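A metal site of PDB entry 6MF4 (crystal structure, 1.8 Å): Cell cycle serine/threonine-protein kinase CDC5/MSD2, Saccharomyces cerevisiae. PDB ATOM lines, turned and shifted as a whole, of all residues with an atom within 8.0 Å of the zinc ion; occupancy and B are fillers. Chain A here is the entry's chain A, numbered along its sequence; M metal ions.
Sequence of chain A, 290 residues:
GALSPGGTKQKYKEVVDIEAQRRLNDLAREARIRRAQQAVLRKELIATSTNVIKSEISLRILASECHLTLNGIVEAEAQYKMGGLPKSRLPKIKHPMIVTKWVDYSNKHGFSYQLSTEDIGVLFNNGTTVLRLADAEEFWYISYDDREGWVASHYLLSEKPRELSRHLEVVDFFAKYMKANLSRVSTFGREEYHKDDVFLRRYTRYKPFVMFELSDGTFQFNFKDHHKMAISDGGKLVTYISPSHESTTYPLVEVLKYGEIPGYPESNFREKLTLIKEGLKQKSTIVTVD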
ATOM      1  N   LEU A 133      -6.078  21.370   9.605  1.00  0.00           N
ATOM      2  CA  LEU A 133      -7.340  20.635   9.570  1.00  0.00           C
ATOM      3  C   LEU A 133      -8.511  21.595   9.551  1.00  0.00           C
ATOM      4  O   LEU A 133      -8.425  22.733  10.001  1.00  0.00           O
ATOM      5  CB  LEU A 133      -7.454  19.688  10.763  1.00  0.00           C
ATOM      6  CG  LEU A 133      -6.793  18.322  10.563  1.00  0.00           C
ATOM      7  CD1 LEU A 133      -5.294  18.438  10.679  1.00  0.00           C
ATOM      8  CD2 LEU A 133      -7.326  17.296  11.546  1.00  0.00           C
ATOM      9  N   ASP A 135     -11.011  21.740  11.248  1.00  0.00           N
ATOM     10  CA  ASP A 135     -11.549  22.103  12.550  1.00  0.00           C
ATOM     11  C   ASP A 135     -10.950  23.417  13.068  1.00  0.00           C
ATOM     12  O   ASP A 135     -11.411  23.967  14.067  1.00  0.00           O
ATOM     13  CB  ASP A 135     -11.314  20.976  13.569  1.00  0.00           C
ATOM     14  CG  ASP A 135      -9.845  20.580  13.699  1.00  0.00           C
ATOM     15  OD1 ASP A 135      -8.955  21.421  13.468  1.00  0.00           O
ATOM     16  OD2 ASP A 135      -9.591  19.419  14.080  1.00  0.00           O
ATOM     17  N   GLU A 137      -8.291  23.909  14.604  1.00  0.00           N
ATOM     18  CA  GLU A 137      -7.615  23.765  15.888  1.00  0.00           C
ATOM     19  C   GLU A 137      -6.359  22.894  15.821  1.00  0.00           C
ATOM     20  O   GLU A 137      -5.424  23.086  16.598  1.00  0.00           O
ATOM     21  CB  GLU A 137      -8.585  23.180  16.943  1.00  0.00           C
ATOM     22  CG  GLU A 137      -7.932  22.671  18.242  1.00  0.00           C
ATOM     23  CD  GLU A 137      -7.080  23.709  18.972  1.00  0.00           C
ATOM     24  OE1 GLU A 137      -6.483  23.350  20.005  1.00  0.00           O
ATOM     25  OE2 GLU A 137      -6.999  24.877  18.529  1.00  0.00           O
ATOM     26  N   GLU A 138      -6.339  21.933  14.891  1.00  0.00           N
ATOM     27  CA  GLU A 138      -5.195  21.038  14.759  1.00  0.00           C
ATOM     28  C   GLU A 138      -4.481  21.228  13.426  1.00  0.00           C
ATOM     29  O   GLU A 138      -5.099  21.575  12.428  1.00  0.00           O
ATOM     30  CB  GLU A 138      -5.631  19.577  14.898  1.00  0.00           C
ATOM     31  CG  GLU A 138      -6.386  19.264  16.181  1.00  0.00           C
ATOM     32  CD  GLU A 138      -6.267  17.806  16.575  1.00  0.00           C
ATOM     33  OE1 GLU A 138      -6.230  16.940  15.685  1.00  0.00           O
ATOM     34  OE2 GLU A 138      -6.204  17.526  17.791  1.00  0.00           O
ATOM     35  N   PHE A 139      -3.167  20.983  13.419  1.00  0.00           N
ATOM     36  CA  PHE A 139      -2.426  20.942  12.168  1.00  0.00           C
ATOM     37  C   PHE A 139      -1.268  19.961  12.248  1.00  0.00           C
ATOM     38  O   PHE A 139      -0.800  19.609  13.335  1.00  0.00           O
ATOM     39  CB  PHE A 139      -1.923  22.346  11.762  1.00  0.00           C
ATOM     40  CG  PHE A 139      -0.789  22.875  12.607  1.00  0.00           C
ATOM     41  CD1 PHE A 139      -1.048  23.603  13.762  1.00  0.00           C
ATOM     42  CD2 PHE A 139       0.530  22.683  12.230  1.00  0.00           C
ATOM     43  CE1 PHE A 139      -0.010  24.112  14.530  1.00  0.00           C
ATOM     44  CE2 PHE A 139       1.567  23.189  12.989  1.00  0.00           C
ATOM     45  CZ  PHE A 139       1.300  23.892  14.153  1.00  0.00           C
ATOM     46  N   TRP A 140      -0.856  19.489  11.072  1.00  0.00           N
ATOM     47  CA  TRP A 140       0.357  18.691  10.905  1.00  0.00           C
ATOM     48  C   TRP A 140       1.468  19.545  10.326  1.00  0.00           C
ATOM     49  O   TRP A 140       1.240  20.294   9.380  1.00  0.00           O
ATOM     50  CB  TRP A 140       0.120  17.512   9.962  1.00  0.00           C
ATOM     51  CG  TRP A 140      -0.847  16.484  10.431  1.00  0.00           C
ATOM     52  CD1 TRP A 140      -2.146  16.357  10.040  1.00  0.00           C
ATOM     53  CD2 TRP A 140      -0.585  15.418  11.342  1.00  0.00           C
ATOM     54  NE1 TRP A 140      -2.721  15.276  10.660  1.00  0.00           N
ATOM     55  CE2 TRP A 140      -1.781  14.684  11.475  1.00  0.00           C
ATOM     56  CE3 TRP A 140       0.530  15.014  12.076  1.00  0.00           C
ATOM     57  CZ2 TRP A 140      -1.895  13.572  12.302  1.00  0.00           C
ATOM     58  CZ3 TRP A 140       0.425  13.903  12.891  1.00  0.00           C
ATOM     59  CH2 TRP A 140      -0.777  13.191  12.996  1.00  0.00           C
ATOM     60  N   HIS A 154       2.161  16.255  14.984  1.00  0.00           N
ATOM     61  CA  HIS A 154       0.826  16.716  15.370  1.00  0.00           C
ATOM     62  C   HIS A 154       0.902  17.923  16.306  1.00  0.00           C
ATOM     63  O   HIS A 154       1.558  17.860  17.339  1.00  0.00           O
ATOM     64  CB  HIS A 154       0.087  15.549  16.035  1.00  0.00           C
ATOM     65  CG  HIS A 154      -1.322  15.847  16.449  1.00  0.00           C
ATOM     66  ND1 HIS A 154      -1.634  16.704  17.474  1.00  0.00           N
ATOM     67  CD2 HIS A 154      -2.501  15.358  15.995  1.00  0.00           C
ATOM     68  CE1 HIS A 154      -2.946  16.749  17.627  1.00  0.00           C
ATOM     69  NE2 HIS A 154      -3.495  15.933  16.749  1.00  0.00           N
ATOM     70  N   TYR A 155       0.229  19.025  15.941  1.00  0.00           N
ATOM     71  CA  TYR A 155       0.195  20.231  16.773  1.00  0.00           C
ATOM     72  C   TYR A 155      -1.205  20.824  16.921  1.00  0.00           C
ATOM     73  O   TYR A 155      -2.098  20.540  16.123  1.00  0.00           O
ATOM     74  CB  TYR A 155       1.106  21.308  16.191  1.00  0.00           C
ATOM     75  CG  TYR A 155       2.579  20.994  16.313  1.00  0.00           C
ATOM     76  CD1 TYR A 155       3.233  21.101  17.529  1.00  0.00           C
ATOM     77  CD2 TYR A 155       3.309  20.611  15.196  1.00  0.00           C
ATOM     78  CE1 TYR A 155       4.576  20.816  17.632  1.00  0.00           C
ATOM     79  CE2 TYR A 155       4.652  20.326  15.299  1.00  0.00           C
ATOM     80  CZ  TYR A 155       5.283  20.433  16.516  1.00  0.00           C
ATOM     81  OH  TYR A 155       6.625  20.145  16.609  1.00  0.00           O
ATOM     82  N   LEU A 156      -1.364  21.649  17.956  1.00  0.00           N
ATOM     83  CA  LEU A 156      -2.560  22.462  18.139  1.00  0.00           C
ATOM     84  C   LEU A 156      -2.234  23.922  17.832  1.00  0.00           C
ATOM     85  O   LEU A 156      -1.176  24.410  18.235  1.00  0.00           O
ATOM     86  CB  LEU A 156      -3.085  22.340  19.572  1.00  0.00           C
ATOM     87  CG  LEU A 156      -3.299  20.933  20.124  1.00  0.00           C
ATOM     88  CD1 LEU A 156      -3.822  21.012  21.549  1.00  0.00           C
ATOM     89  CD2 LEU A 156      -4.269  20.147  19.242  1.00  0.00           C
ATOM     90  N   PHE A 188       0.345   9.649   9.246  1.00  0.00           N
ATOM     91  CA  PHE A 188      -0.499  10.349  10.219  1.00  0.00           C
ATOM     92  C   PHE A 188      -1.057   9.452  11.337  1.00  0.00           C
ATOM     93  O   PHE A 188      -1.987   9.853  12.036  1.00  0.00           O
ATOM     94  CB  PHE A 188      -1.657  11.031   9.492  1.00  0.00           C
ATOM     95  CG  PHE A 188      -1.210  11.993   8.428  1.00  0.00           C
ATOM     96  CD1 PHE A 188      -0.596  13.181   8.767  1.00  0.00           C
ATOM     97  CD2 PHE A 188      -1.426  11.706   7.099  1.00  0.00           C
ATOM     98  CE1 PHE A 188      -0.182  14.058   7.786  1.00  0.00           C
ATOM     99  CE2 PHE A 188      -1.026  12.584   6.108  1.00  0.00           C
ATOM    100  CZ  PHE A 188      -0.393  13.763   6.460  1.00  0.00           C
ATOM    101  N   GLU A 191      -5.036   6.941  14.778  1.00  0.00           N
ATOM    102  CA  GLU A 191      -6.142   7.536  15.526  1.00  0.00           C
ATOM    103  C   GLU A 191      -7.326   7.744  14.577  1.00  0.00           C
ATOM    104  O   GLU A 191      -7.124   8.052  13.401  1.00  0.00           O
ATOM    105  CB  GLU A 191      -5.724   8.855  16.172  1.00  0.00           C
ATOM    106  CG  GLU A 191      -5.287   8.737  17.632  1.00  0.00           C
ATOM    107  CD  GLU A 191      -6.459   8.832  18.594  1.00  0.00           C
ATOM    108  OE1 GLU A 191      -7.010   9.939  18.767  1.00  0.00           O
ATOM    109  OE2 GLU A 191      -6.834   7.793  19.186  1.00  0.00           O
ATOM    110  N   TYR A 193      -9.512  10.047  14.197  1.00  0.00           N
ATOM    111  CA  TYR A 193      -9.672  11.393  13.652  1.00  0.00           C
ATOM    112  C   TYR A 193      -8.700  11.686  12.511  1.00  0.00           C
ATOM    113  O   TYR A 193      -8.914  12.641  11.757  1.00  0.00           O
ATOM    114  CB  TYR A 193      -9.469  12.415  14.780  1.00  0.00           C
ATOM    115  CG  TYR A 193     -10.014  13.805  14.522  1.00  0.00           C
ATOM    116  CD1 TYR A 193     -11.379  14.031  14.388  1.00  0.00           C
ATOM    117  CD2 TYR A 193      -9.160  14.906  14.474  1.00  0.00           C
ATOM    118  CE1 TYR A 193     -11.881  15.303  14.172  1.00  0.00           C
ATOM    119  CE2 TYR A 193      -9.653  16.186  14.266  1.00  0.00           C
ATOM    120  CZ  TYR A 193     -11.013  16.376  14.123  1.00  0.00           C
ATOM    121  OH  TYR A 193     -11.502  17.641  13.899  1.00  0.00           O
ATOM    122  N   HIS A 194      -7.669  10.855  12.369  1.00  0.00           N
ATOM    123  CA  HIS A 194      -6.563  11.141  11.441  1.00  0.00           C
ATOM    124  C   HIS A 194      -6.293  10.047  10.417  1.00  0.00           C
ATOM    125  O   HIS A 194      -5.445  10.232   9.540  1.00  0.00           O
ATOM    126  CB  HIS A 194      -5.285  11.397  12.233  1.00  0.00           C
ATOM    127  CG  HIS A 194      -5.315  12.655  13.035  1.00  0.00           C
ATOM    128  ND1 HIS A 194      -5.506  13.891  12.466  1.00  0.00           N
ATOM    129  CD2 HIS A 194      -5.197  12.866  14.371  1.00  0.00           C
ATOM    130  CE1 HIS A 194      -5.494  14.815  13.409  1.00  0.00           C
ATOM    131  NE2 HIS A 194      -5.307  14.217  14.578  1.00  0.00           N
ATOM    132  N   ASP A 197      -6.254  10.998   6.833  1.00  0.00           N
ATOM    133  CA  ASP A 197      -5.585  12.268   6.536  1.00  0.00           C
ATOM    134  C   ASP A 197      -4.686  12.120   5.311  1.00  0.00           C
ATOM    135  O   ASP A 197      -4.052  11.089   5.119  1.00  0.00           O
ATOM    136  CB  ASP A 197      -4.771  12.758   7.740  1.00  0.00           C
ATOM    137  CG  ASP A 197      -5.642  13.354   8.835  1.00  0.00           C
ATOM    138  OD1 ASP A 197      -6.890  13.224   8.763  1.00  0.00           O
ATOM    139  OD2 ASP A 197      -5.081  13.960   9.778  1.00  0.00           O
HETATM  140 ZN    ZN M   1      -5.411  15.240  16.295  1.00  0.00          ZN
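N of Leu 133 lies within hydrogen-bond range of O of Glu 138 (3.0 Å).
The side-chain carboxylate (OD1) of Asp 135 lies within hydrogen-bond range of the backbone NH (N) of Glu 138, 3.0 Å away.
OD2 of Asp 197 is in hydrogen-bond range of ND1 of His 194, at 2.7 Å.
Of the 14 residues printed, 3 come within 4 Å of the zinc ion.
OE1 of Glu 138 binds the zinc ion (2.0 Å).
The zinc ion is bound by NE2 of His 194 (2.0 Å).
The zinc ion is bound by a ring nitrogen (NE2) of His 154 (2.1 Å).
Slightly farther from the zinc ion lies the side-chain carboxylate (OE2) of Glu 138 (2.8 Å).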
